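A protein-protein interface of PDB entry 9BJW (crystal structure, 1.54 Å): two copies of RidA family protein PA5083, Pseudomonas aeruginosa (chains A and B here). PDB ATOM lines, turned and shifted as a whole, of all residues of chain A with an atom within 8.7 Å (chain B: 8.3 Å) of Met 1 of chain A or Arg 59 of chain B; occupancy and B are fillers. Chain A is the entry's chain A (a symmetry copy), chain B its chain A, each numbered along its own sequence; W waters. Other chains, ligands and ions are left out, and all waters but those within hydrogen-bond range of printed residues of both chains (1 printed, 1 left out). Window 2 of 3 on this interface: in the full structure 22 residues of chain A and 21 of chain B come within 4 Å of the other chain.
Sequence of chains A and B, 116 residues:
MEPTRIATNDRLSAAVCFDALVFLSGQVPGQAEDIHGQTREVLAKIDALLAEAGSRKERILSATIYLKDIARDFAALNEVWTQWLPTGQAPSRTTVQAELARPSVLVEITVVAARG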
ATOM      1  N   MET A   1     -34.196 -15.839  -6.482  1.00  0.00           N
ATOM      2  CA  MET A   1     -33.178 -15.441  -5.522  1.00  0.00           C
ATOM      3  C   MET A   1     -33.139 -16.399  -4.337  1.00  0.00           C
ATOM      4  O   MET A   1     -32.070 -16.668  -3.798  1.00  0.00           O
ATOM      5  CB  MET A   1     -33.425 -14.009  -5.036  1.00  0.00           C
ATOM      6  CG  MET A   1     -32.337 -13.462  -4.108  1.00  0.00           C
ATOM      7  SD  MET A   1     -32.680 -13.655  -2.340  1.00  0.00           S
ATOM      8  CE  MET A   1     -33.629 -12.169  -2.004  1.00  0.00           C
ATOM      9  N   GLU A   2     -34.320 -16.913  -3.930  1.00  0.00           N
ATOM     10  CA  GLU A   2     -34.425 -17.796  -2.777  1.00  0.00           C
ATOM     11  C   GLU A   2     -34.759 -19.216  -3.213  1.00  0.00           C
ATOM     12  O   GLU A   2     -35.575 -19.404  -4.121  1.00  0.00           O
ATOM     13  CB  GLU A   2     -35.506 -17.320  -1.794  1.00  0.00           C
ATOM     14  CG  GLU A   2     -35.312 -15.903  -1.263  1.00  0.00           C
ATOM     15  CD  GLU A   2     -35.948 -14.853  -2.150  1.00  0.00           C
ATOM     16  OE1 GLU A   2     -36.464 -13.847  -1.616  1.00  0.00           O
ATOM     17  OE2 GLU A   2     -35.952 -15.040  -3.383  1.00  0.00           O
ATOM     18  N   PRO A   3     -34.144 -20.225  -2.600  1.00  0.00           N
ATOM     19  CA  PRO A   3     -34.624 -21.597  -2.804  1.00  0.00           C
ATOM     20  C   PRO A   3     -35.992 -21.774  -2.163  1.00  0.00           C
ATOM     21  O   PRO A   3     -36.283 -21.191  -1.116  1.00  0.00           O
ATOM     22  CB  PRO A   3     -33.567 -22.465  -2.105  1.00  0.00           C
ATOM     23  CG  PRO A   3     -32.399 -21.562  -1.856  1.00  0.00           C
ATOM     24  CD  PRO A   3     -32.950 -20.174  -1.743  1.00  0.00           C
ATOM     25  N   THR A   4     -36.835 -22.576  -2.804  1.00  0.00           N
ATOM     26  CA  THR A   4     -38.119 -22.959  -2.238  1.00  0.00           C
ATOM     27  C   THR A   4     -38.136 -24.466  -2.034  1.00  0.00           C
ATOM     28  O   THR A   4     -37.358 -25.205  -2.646  1.00  0.00           O
ATOM     29  CB  THR A   4     -39.297 -22.526  -3.121  1.00  0.00           C
ATOM     30  OG1 THR A   4     -39.149 -23.062  -4.440  1.00  0.00           O
ATOM     31  CG2 THR A   4     -39.369 -21.000  -3.192  1.00  0.00           C
ATOM     32  N   ARG A   5     -39.023 -24.919  -1.154  1.00  0.00           N
ATOM     33  CA  ARG A   5     -38.985 -26.297  -0.687  1.00  0.00           C
ATOM     34  C   ARG A   5     -40.357 -26.951  -0.783  1.00  0.00           C
ATOM     35  O   ARG A   5     -41.393 -26.292  -0.658  1.00  0.00           O
ATOM     36  CB  ARG A   5     -38.477 -26.361   0.753  1.00  0.00           C
ATOM     37  CG  ARG A   5     -37.099 -25.751   0.939  1.00  0.00           C
ATOM     38  CD  ARG A   5     -36.623 -25.837   2.375  1.00  0.00           C
ATOM     39  NE  ARG A   5     -35.319 -25.200   2.509  1.00  0.00           N
ATOM     40  CZ  ARG A   5     -35.141 -23.899   2.677  1.00  0.00           C
ATOM     41  NH1 ARG A   5     -36.167 -23.076   2.822  1.00  0.00           N
ATOM     42  NH2 ARG A   5     -33.903 -23.412   2.696  1.00  0.00           N
ATOM     43  N   VAL A  16     -36.084 -29.383  -3.441  1.00  0.00           N
ATOM     44  CA  VAL A  16     -35.656 -27.997  -3.295  1.00  0.00           C
ATOM     45  C   VAL A  16     -35.486 -27.412  -4.686  1.00  0.00           C
ATOM     46  O   VAL A  16     -34.802 -27.996  -5.534  1.00  0.00           O
ATOM     47  CB  VAL A  16     -34.359 -27.864  -2.480  1.00  0.00           C
ATOM     48  CG1 VAL A  16     -33.886 -26.414  -2.480  1.00  0.00           C
ATOM     49  CG2 VAL A  16     -34.573 -28.348  -1.060  1.00  0.00           C
ATOM     50  N   CYS A  17     -36.123 -26.273  -4.926  1.00  0.00           N
ATOM     51  CA  CYS A  17     -36.070 -25.603  -6.214  1.00  0.00           C
ATOM     52  C   CYS A  17     -35.249 -24.327  -6.095  1.00  0.00           C
ATOM     53  O   CYS A  17     -35.377 -23.586  -5.116  1.00  0.00           O
ATOM     54  CB  CYS A  17     -37.476 -25.266  -6.720  1.00  0.00           C
ATOM     55  SG  CYS A  17     -38.550 -26.721  -6.850  1.00  0.00           S
ATOM     56  N   PHE A  18     -34.400 -24.088  -7.085  1.00  0.00           N
ATOM     57  CA  PHE A  18     -33.615 -22.860  -7.131  1.00  0.00           C
ATOM     58  C   PHE A  18     -33.438 -22.467  -8.583  1.00  0.00           C
ATOM     59  O   PHE A  18     -32.864 -23.228  -9.368  1.00  0.00           O
ATOM     60  CB  PHE A  18     -32.259 -23.017  -6.443  1.00  0.00           C
ATOM     61  CG  PHE A  18     -31.454 -21.750  -6.433  1.00  0.00           C
ATOM     62  CD1 PHE A  18     -31.901 -20.642  -5.728  1.00  0.00           C
ATOM     63  CD2 PHE A  18     -30.276 -21.653  -7.149  1.00  0.00           C
ATOM     64  CE1 PHE A  18     -31.175 -19.461  -5.730  1.00  0.00           C
ATOM     65  CE2 PHE A  18     -29.545 -20.475  -7.150  1.00  0.00           C
ATOM     66  CZ  PHE A  18     -29.998 -19.382  -6.437  1.00  0.00           C
ATOM     67  N   ASP A  19     -33.932 -21.275  -8.922  1.00  0.00           N
ATOM     68  CA  ASP A  19     -34.025 -20.825 -10.300  1.00  0.00           C
ATOM     69  C   ASP A  19     -34.690 -21.895 -11.154  1.00  0.00           C
ATOM     70  O   ASP A  19     -35.832 -22.280 -10.891  1.00  0.00           O
ATOM     71  CB  ASP A  19     -32.645 -20.464 -10.844  1.00  0.00           C
ATOM     72  CG  ASP A  19     -32.707 -19.392 -11.922  1.00  0.00           C
ATOM     73  OD1 ASP A  19     -33.821 -19.066 -12.393  1.00  0.00           O
ATOM     74  OD2 ASP A  19     -31.636 -18.868 -12.291  1.00  0.00           O
ATOM     75  N   ALA A  20     -33.984 -22.389 -12.168  1.00  0.00           N
ATOM     76  CA  ALA A  20     -34.542 -23.370 -13.088  1.00  0.00           C
ATOM     77  C   ALA A  20     -34.163 -24.798 -12.726  1.00  0.00           C
ATOM     78  O   ALA A  20     -34.353 -25.697 -13.549  1.00  0.00           O
ATOM     79  CB  ALA A  20     -34.101 -23.067 -14.518  1.00  0.00           C
ATOM     80  N   PHE A  23     -33.863 -30.042  -7.187  1.00  0.00           N
ATOM     81  CA  PHE A  23     -33.053 -31.060  -6.513  1.00  0.00           C
ATOM     82  C   PHE A  23     -33.970 -31.946  -5.675  1.00  0.00           C
ATOM     83  O   PHE A  23     -34.590 -31.475  -4.719  1.00  0.00           O
ATOM     84  CB  PHE A  23     -31.989 -30.416  -5.615  1.00  0.00           C
ATOM     85  CG  PHE A  23     -30.999 -29.550  -6.351  1.00  0.00           C
ATOM     86  CD1 PHE A  23     -31.343 -28.260  -6.736  1.00  0.00           C
ATOM     87  CD2 PHE A  23     -29.718 -30.016  -6.629  1.00  0.00           C
ATOM     88  CE1 PHE A  23     -30.433 -27.452  -7.417  1.00  0.00           C
ATOM     89  CE2 PHE A  23     -28.800 -29.205  -7.303  1.00  0.00           C
ATOM     90  CZ  PHE A  23     -29.166 -27.922  -7.692  1.00  0.00           C
ATOM     91  N   ALA B  20     -24.615 -18.648  -9.601  1.00  0.00           N
ATOM     92  CA  ALA B  20     -25.254 -18.624  -8.295  1.00  0.00           C
ATOM     93  C   ALA B  20     -25.130 -19.947  -7.554  1.00  0.00           C
ATOM     94  O   ALA B  20     -25.831 -20.147  -6.559  1.00  0.00           O
ATOM     95  CB  ALA B  20     -26.728 -18.247  -8.431  1.00  0.00           C
ATOM     96  N   LEU B  21     -24.263 -20.843  -8.011  1.00  0.00           N
ATOM     97  CA  LEU B  21     -24.122 -22.160  -7.402  1.00  0.00           C
ATOM     98  C   LEU B  21     -22.767 -22.307  -6.722  1.00  0.00           C
ATOM     99  O   LEU B  21     -21.750 -21.770  -7.179  1.00  0.00           O
ATOM    100  CB  LEU B  21     -24.286 -23.274  -8.443  1.00  0.00           C
ATOM    101  CG  LEU B  21     -25.683 -23.366  -9.067  1.00  0.00           C
ATOM    102  CD1 LEU B  21     -25.688 -24.440 -10.159  1.00  0.00           C
ATOM    103  CD2 LEU B  21     -26.720 -23.672  -8.002  1.00  0.00           C
ATOM    104  N   VAL B  22     -22.768 -23.064  -5.629  1.00  0.00           N
ATOM    105  CA  VAL B  22     -21.579 -23.367  -4.854  1.00  0.00           C
ATOM    106  C   VAL B  22     -21.493 -24.884  -4.749  1.00  0.00           C
ATOM    107  O   VAL B  22     -22.427 -25.520  -4.245  1.00  0.00           O
ATOM    108  CB  VAL B  22     -21.631 -22.732  -3.455  1.00  0.00           C
ATOM    109  CG1 VAL B  22     -20.405 -23.124  -2.655  1.00  0.00           C
ATOM    110  CG2 VAL B  22     -21.804 -21.196  -3.557  1.00  0.00           C
ATOM    111  N   LEU B  50     -19.408 -22.632   3.225  1.00  0.00           N
ATOM    112  CA  LEU B  50     -20.553 -21.865   2.742  1.00  0.00           C
ATOM    113  C   LEU B  50     -20.334 -20.377   2.970  1.00  0.00           C
ATOM    114  O   LEU B  50     -20.556 -19.560   2.068  1.00  0.00           O
ATOM    115  CB  LEU B  50     -21.836 -22.323   3.433  1.00  0.00           C
ATOM    116  CG  LEU B  50     -22.299 -23.743   3.086  1.00  0.00           C
ATOM    117  CD1 LEU B  50     -23.512 -24.103   3.924  1.00  0.00           C
ATOM    118  CD2 LEU B  50     -22.618 -23.810   1.598  1.00  0.00           C
ATOM    119  N   GLY B  54     -19.949 -17.189  -0.038  1.00  0.00           N
ATOM    120  CA  GLY B  54     -21.106 -16.333  -0.194  1.00  0.00           C
ATOM    121  C   GLY B  54     -22.441 -17.023  -0.052  1.00  0.00           C
ATOM    122  O   GLY B  54     -23.442 -16.523  -0.580  1.00  0.00           O
ATOM    123  N   SER B  55     -22.494 -18.160   0.638  1.00  0.00           N
ATOM    124  CA  SER B  55     -23.740 -18.869   0.904  1.00  0.00           C
ATOM    125  C   SER B  55     -23.958 -18.964   2.418  1.00  0.00           C
ATOM    126  O   SER B  55     -23.296 -18.279   3.204  1.00  0.00           O
ATOM    127  CB  SER B  55     -23.715 -20.251   0.237  1.00  0.00           C
ATOM    128  OG  SER B  55     -25.003 -20.845   0.238  1.00  0.00           O
ATOM    129  N   ARG B  56     -24.878 -19.839   2.825  1.00  0.00           N
ATOM    130  CA  ARG B  56     -25.234 -20.028   4.229  1.00  0.00           C
ATOM    131  C   ARG B  56     -26.051 -21.312   4.334  1.00  0.00           C
ATOM    132  O   ARG B  56     -26.500 -21.855   3.320  1.00  0.00           O
ATOM    133  CB  ARG B  56     -26.011 -18.821   4.777  1.00  0.00           C
ATOM    134  CG  ARG B  56     -27.262 -18.477   3.982  1.00  0.00           C
ATOM    135  CD  ARG B  56     -27.867 -17.143   4.431  1.00  0.00           C
ATOM    136  NE  ARG B  56     -28.254 -17.170   5.836  1.00  0.00           N
ATOM    137  CZ  ARG B  56     -28.800 -16.145   6.480  1.00  0.00           C
ATOM    138  NH1 ARG B  56     -29.047 -14.999   5.866  1.00  0.00           N
ATOM    139  NH2 ARG B  56     -29.104 -16.276   7.768  1.00  0.00           N
ATOM    140  N   LYS B  57     -26.248 -21.787   5.575  1.00  0.00           N
ATOM    141  CA  LYS B  57     -26.982 -23.040   5.782  1.00  0.00           C
ATOM    142  C   LYS B  57     -28.361 -22.992   5.148  1.00  0.00           C
ATOM    143  O   LYS B  57     -28.820 -23.985   4.571  1.00  0.00           O
ATOM    144  CB  LYS B  57     -27.148 -23.361   7.270  1.00  0.00           C
ATOM    145  CG  LYS B  57     -25.898 -23.491   8.046  1.00  0.00           C
ATOM    146  CD  LYS B  57     -26.132 -24.258   9.340  1.00  0.00           C
ATOM    147  CE  LYS B  57     -26.049 -23.349  10.546  1.00  0.00           C
ATOM    148  NZ  LYS B  57     -26.051 -24.174  11.795  1.00  0.00           N
ATOM    149  N   GLU B  58     -29.043 -21.845   5.249  1.00  0.00           N
ATOM    150  CA  GLU B  58     -30.396 -21.719   4.732  1.00  0.00           C
ATOM    151  C   GLU B  58     -30.464 -21.828   3.218  1.00  0.00           C
ATOM    152  O   GLU B  58     -31.571 -21.871   2.665  1.00  0.00           O
ATOM    153  CB  GLU B  58     -30.998 -20.373   5.156  1.00  0.00           C
ATOM    154  CG  GLU B  58     -31.215 -20.200   6.642  1.00  0.00           C
ATOM    155  CD  GLU B  58     -29.955 -19.832   7.417  1.00  0.00           C
ATOM    156  OE1 GLU B  58     -28.834 -19.799   6.845  1.00  0.00           O
ATOM    157  OE2 GLU B  58     -30.076 -19.587   8.636  1.00  0.00           O
ATOM    158  N   ARG B  59     -29.322 -21.829   2.532  1.00  0.00           N
ATOM    159  CA  ARG B  59     -29.297 -21.865   1.079  1.00  0.00           C
ATOM    160  C   ARG B  59     -28.698 -23.155   0.535  1.00  0.00           C
ATOM    161  O   ARG B  59     -28.386 -23.226  -0.655  1.00  0.00           O
ATOM    162  CB  ARG B  59     -28.547 -20.649   0.543  1.00  0.00           C
ATOM    163  CG  ARG B  59     -29.284 -19.345   0.869  1.00  0.00           C
ATOM    164  CD  ARG B  59     -28.604 -18.109   0.294  1.00  0.00           C
ATOM    165  NE  ARG B  59     -28.715 -18.023  -1.156  1.00  0.00           N
ATOM    166  CZ  ARG B  59     -29.735 -17.476  -1.805  1.00  0.00           C
ATOM    167  NH1 ARG B  59     -30.797 -17.014  -1.165  1.00  0.00           N
ATOM    168  NH2 ARG B  59     -29.689 -17.395  -3.131  1.00  0.00           N
ATOM    169  N   ILE B  60     -28.540 -24.179   1.375  1.00  0.00           N
ATOM    170  CA  ILE B  60     -28.142 -25.493   0.879  1.00  0.00           C
ATOM    171  C   ILE B  60     -29.240 -26.045  -0.018  1.00  0.00           C
ATOM    172  O   ILE B  60     -30.430 -25.991   0.320  1.00  0.00           O
ATOM    173  CB  ILE B  60     -27.854 -26.445   2.046  1.00  0.00           C
ATOM    174  CG1 ILE B  60     -26.735 -25.891   2.927  1.00  0.00           C
ATOM    175  CG2 ILE B  60     -27.479 -27.833   1.525  1.00  0.00           C
ATOM    176  CD1 ILE B  60     -26.584 -26.625   4.264  1.00  0.00           C
ATOM    177  N   LEU B  61     -28.842 -26.587  -1.168  1.00  0.00           N
ATOM    178  CA  LEU B  61     -29.761 -27.186  -2.122  1.00  0.00           C
ATOM    179  C   LEU B  61     -29.810 -28.701  -2.006  1.00  0.00           C
ATOM    180  O   LEU B  61     -30.900 -29.288  -2.037  1.00  0.00           O
ATOM    181  CB  LEU B  61     -29.362 -26.786  -3.548  1.00  0.00           C
ATOM    182  CG  LEU B  61     -29.339 -25.273  -3.786  1.00  0.00           C
ATOM    183  CD1 LEU B  61     -28.835 -24.958  -5.184  1.00  0.00           C
ATOM    184  CD2 LEU B  61     -30.717 -24.660  -3.558  1.00  0.00           C
ATOM    185  N   SER B  62     -28.651 -29.332  -1.839  1.00  0.00           N
ATOM    186  CA  SER B  62     -28.576 -30.782  -1.741  1.00  0.00           C
ATOM    187  C   SER B  62     -27.408 -31.180  -0.854  1.00  0.00           C
ATOM    188  O   SER B  62     -26.369 -30.511  -0.814  1.00  0.00           O
ATOM    189  CB  SER B  62     -28.408 -31.417  -3.127  1.00  0.00           C
ATOM    190  OG  SER B  62     -27.161 -31.041  -3.693  1.00  0.00           O
ATOM    191  N   PRO B  86     -30.916 -25.097  10.022  1.00  0.00           N
ATOM    192  CA  PRO B  86     -31.867 -24.025  10.350  1.00  0.00           C
ATOM    193  C   PRO B  86     -33.295 -24.555  10.350  1.00  0.00           C
ATOM    194  O   PRO B  86     -33.693 -25.318   9.467  1.00  0.00           O
ATOM    195  CB  PRO B  86     -31.641 -22.991   9.240  1.00  0.00           C
ATOM    196  CG  PRO B  86     -30.972 -23.753   8.122  1.00  0.00           C
ATOM    197  CD  PRO B  86     -30.186 -24.853   8.766  1.00  0.00           C
ATOM    198  N   GLN B  89     -35.924 -25.385   7.329  1.00  0.00           N
ATOM    199  CA  GLN B  89     -35.256 -25.047   6.073  1.00  0.00           C
ATOM    200  C   GLN B  89     -34.310 -26.156   5.625  1.00  0.00           C
ATOM    201  O   GLN B  89     -33.219 -25.898   5.107  1.00  0.00           O
ATOM    202  CB  GLN B  89     -34.524 -23.714   6.203  1.00  0.00           C
ATOM    203  CG  GLN B  89     -35.470 -22.566   6.570  1.00  0.00           C
ATOM    204  CD  GLN B  89     -34.736 -21.300   6.958  1.00  0.00           C
ATOM    205  OE1 GLN B  89     -34.459 -20.455   6.117  1.00  0.00           O
ATOM    206  NE2 GLN B  89     -34.418 -21.167   8.240  1.00  0.00           N
ATOM    207  N   ALA B  90     -34.718 -27.413   5.799  1.00  0.00           N
ATOM    208  CA  ALA B  90     -33.841 -28.521   5.455  1.00  0.00           C
ATOM    209  C   ALA B  90     -33.687 -28.653   3.940  1.00  0.00           C
ATOM    210  O   ALA B  90     -34.625 -28.392   3.181  1.00  0.00           O
ATOM    211  CB  ALA B  90     -34.365 -29.830   6.037  1.00  0.00           C
ATOM    212  N   PRO B  91     -32.500 -29.082   3.481  1.00  0.00           N
ATOM    213  CA  PRO B  91     -32.250 -29.230   2.041  1.00  0.00           C
ATOM    214  C   PRO B  91     -32.703 -30.586   1.512  1.00  0.00           C
ATOM    215  O   PRO B  91     -33.137 -31.438   2.295  1.00  0.00           O
ATOM    216  CB  PRO B  91     -30.725 -29.100   1.962  1.00  0.00           C
ATOM    217  CG  PRO B  91     -30.276 -29.819   3.235  1.00  0.00           C
ATOM    218  CD  PRO B  91     -31.308 -29.419   4.281  1.00  0.00           C
ATOM    219  N   VAL B 111     -22.005 -31.153  -0.297  1.00  0.00           N
ATOM    220  CA  VAL B 111     -23.068 -30.154  -0.365  1.00  0.00           C
ATOM    221  C   VAL B 111     -22.977 -29.327  -1.652  1.00  0.00           C
ATOM    222  O   VAL B 111     -21.886 -28.962  -2.102  1.00  0.00           O
ATOM    223  CB  VAL B 111     -23.023 -29.231   0.879  1.00  0.00           C
ATOM    224  CG1 VAL B 111     -23.661 -27.868   0.610  1.00  0.00           C
ATOM    225  CG2 VAL B 111     -23.711 -29.917   2.073  1.00  0.00           C
ATOM    226  N   VAL B 112     -24.138 -29.063  -2.247  1.00  0.00           N
ATOM    227  CA  VAL B 112     -24.321 -28.022  -3.260  1.00  0.00           C
ATOM    228  C   VAL B 112     -25.280 -26.993  -2.676  1.00  0.00           C
ATOM    229  O   VAL B 112     -26.290 -27.359  -2.061  1.00  0.00           O
ATOM    230  CB  VAL B 112     -24.865 -28.592  -4.587  1.00  0.00           C
ATOM    231  CG1 VAL B 112     -25.041 -27.463  -5.653  1.00  0.00           C
ATOM    232  CG2 VAL B 112     -23.956 -29.684  -5.121  1.00  0.00           C
ATOM    233  N   ALA B 113     -24.979 -25.700  -2.876  1.00  0.00           N
ATOM    234  CA  ALA B 113     -25.755 -24.623  -2.271  1.00  0.00           C
ATOM    235  C   ALA B 113     -25.880 -23.451  -3.236  1.00  0.00           C
ATOM    236  O   ALA B 113     -25.200 -23.379  -4.260  1.00  0.00           O
ATOM    237  CB  ALA B 113     -25.119 -24.147  -0.963  1.00  0.00           C
ATOM    238  N   ALA B 114     -26.747 -22.509  -2.865  1.00  0.00           N
ATOM    239  CA  ALA B 114     -27.023 -21.319  -3.663  1.00  0.00           C
ATOM    240  C   ALA B 114     -26.286 -20.123  -3.081  1.00  0.00           C
ATOM    241  O   ALA B 114     -26.342 -19.883  -1.871  1.00  0.00           O
ATOM    242  CB  ALA B 114     -28.523 -21.036  -3.703  1.00  0.00           C
ATOM    243  N   ARG B 115     -25.592 -19.387  -3.947  1.00  0.00           N
ATOM    244  CA  ARG B 115     -25.024 -18.102  -3.562  1.00  0.00           C
ATOM    245  C   ARG B 115     -26.131 -17.167  -3.100  1.00  0.00           C
ATOM    246  O   ARG B 115     -27.231 -17.159  -3.661  1.00  0.00           O
ATOM    247  CB  ARG B 115     -24.292 -17.473  -4.744  1.00  0.00           C
ATOM    248  CG  ARG B 115     -23.076 -18.221  -5.222  1.00  0.00           C
ATOM    249  CD  ARG B 115     -21.828 -17.652  -4.594  1.00  0.00           C
ATOM    250  NE  ARG B 115     -20.672 -17.727  -5.476  1.00  0.00           N
ATOM    251  CZ  ARG B 115     -20.245 -16.715  -6.218  1.00  0.00           C
ATOM    252  NH1 ARG B 115     -20.829 -15.528  -6.167  1.00  0.00           N
ATOM    253  NH2 ARG B 115     -19.197 -16.891  -7.018  1.00  0.00           N
ATOM    254  N   GLY B 116     -25.834 -16.365  -2.082  1.00  0.00           N
ATOM    255  CA  GLY B 116     -26.776 -15.373  -1.593  1.00  0.00           C
ATOM    256  C   GLY B 116     -26.690 -14.077  -2.372  1.00  0.00           C
ATOM    257  O   GLY B 116     -26.007 -14.001  -3.397  1.00  0.00           O
HETATM  258  O   HOH W   1     -32.312 -25.749   2.184  1.00  0.00           O
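Water W1 lies within hydrogen-bond range of the backbone carbonyl oxygen (O) of Ile 60 of chain B (2.7 Å), the guanidinium group (NH2) of Arg 5 of chain A (2.9 Å) and the backbone carbonyl oxygen (O) of Gln 89 of chain B (3.1 Å).
The backbone carbonyl oxygen of Glu 58 of chain B sits at hydrogen-bond distance from the guanidinium group of Arg 5 of chain A, 2.8 Å away. The guanidinium group (NH2) of Arg 59 of chain B is in hydrogen-bond range of the backbone carbonyl oxygen (O) of Met 1 of chain A. O of Gln 89 of chain B lies close to NE of Arg 5 of chain A (3.4 Å). The guanidinium group (NE) of Arg 5 of chain A sits at hydrogen-bond distance from the backbone carbonyl oxygen (O) of Ala 90 of chain B, 3.3 Å away.
Met 1 of chain A touches one residue of chain B. Glu 2 of chain A touches none of the printed residues of chain B. Of chain A, only Met 1, Pro 3 and Phe 18 come within 4 Å of Arg 59 of chain B. Of the printed residues of chain A, Ser 62 of chain B touches Phe 23 (3.99 Å). Of the printed residues of chain A, Ala 90 of chain B touches Arg 5 (3.3 Å). Of chain A, only Phe 18 comes within 4 Å of Ala 114 of chain B. The nearest residue of chain A that does not touch Arg 59 of chain B is Glu 2 of chain A (4.05 Å). The nearest printed residue of chain B that does not touch Phe 18 of chain A is Leu 21 of chain B (4.2 Å).
Of the 23 printed residues of chain B, 9 touch a printed residue of chain A. Hydrophobic or aromatic side chains of chain B within 4 Å of the printed part of chain A: Ala 20, Leu 61 and Ala 114. Among the printed residues, 14 pairs touch across the chains. Among the printed residues, no Asp or Glu carboxylate lies within 4 Å of a Lys or Arg side-chain nitrogen of the other chain.
Among the printed residues, pairs that only touch across the chains: Pro 3 of chain A with Arg 59 of chain B (3.9 Å), Pro 3 of chain A with Leu 61 of chain B (3.9 Å), Val 16 of chain A with Leu 61 of chain B (3.8 Å), Val 16 of chain A with Pro 91 of chain B (3.9 Å), Phe 18 of chain A with Ala 20 of chain B (3.8 Å), Phe 18 of chain A with Arg 59 of chain B (3.6 Å), Phe 18 of chain A with Leu 61 of chain B (3.7 Å), Phe 18 of chain A with Ala 114 of chain B (3.5 Å), Phe 23 of chain A with Leu 61 of chain B (3.7 Å) and Phe 23 of chain A with Ser 62 of chain B (3.99 Å).
OG of Ser 55 of chain B lies within hydrogen-bond range of O of Ala 114 of chain B (2.7 Å). The side-chain carboxylate (OE1) of Glu 58 of chain B is in salt-bridge range of the guanidinium group (NE) of Arg 56 of chain B, 2.9 Å away. O of Arg 59 of chain B sits at hydrogen-bond distance from N of Ala 114 of chain B, at 2.8 Å. O of Arg 115 of chain B lies within hydrogen-bond range of NH2 of Arg 59 of chain B (2.5 Å). The backbone carbonyl oxygen (O) of Ser 62 of chain B sits at hydrogen-bond distance from the backbone NH (N) of Val 112 of chain B (3.0 Å). The backbone NH of Phe 23 of chain A lies within hydrogen-bond range of the backbone carbonyl oxygen of Val 16 of chain A (2.8 Å).
Position printed for both chains: 20. Of the 14 pairs that touch across the chains among the printed residues, none has its exchanged pair printed and touching as well.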
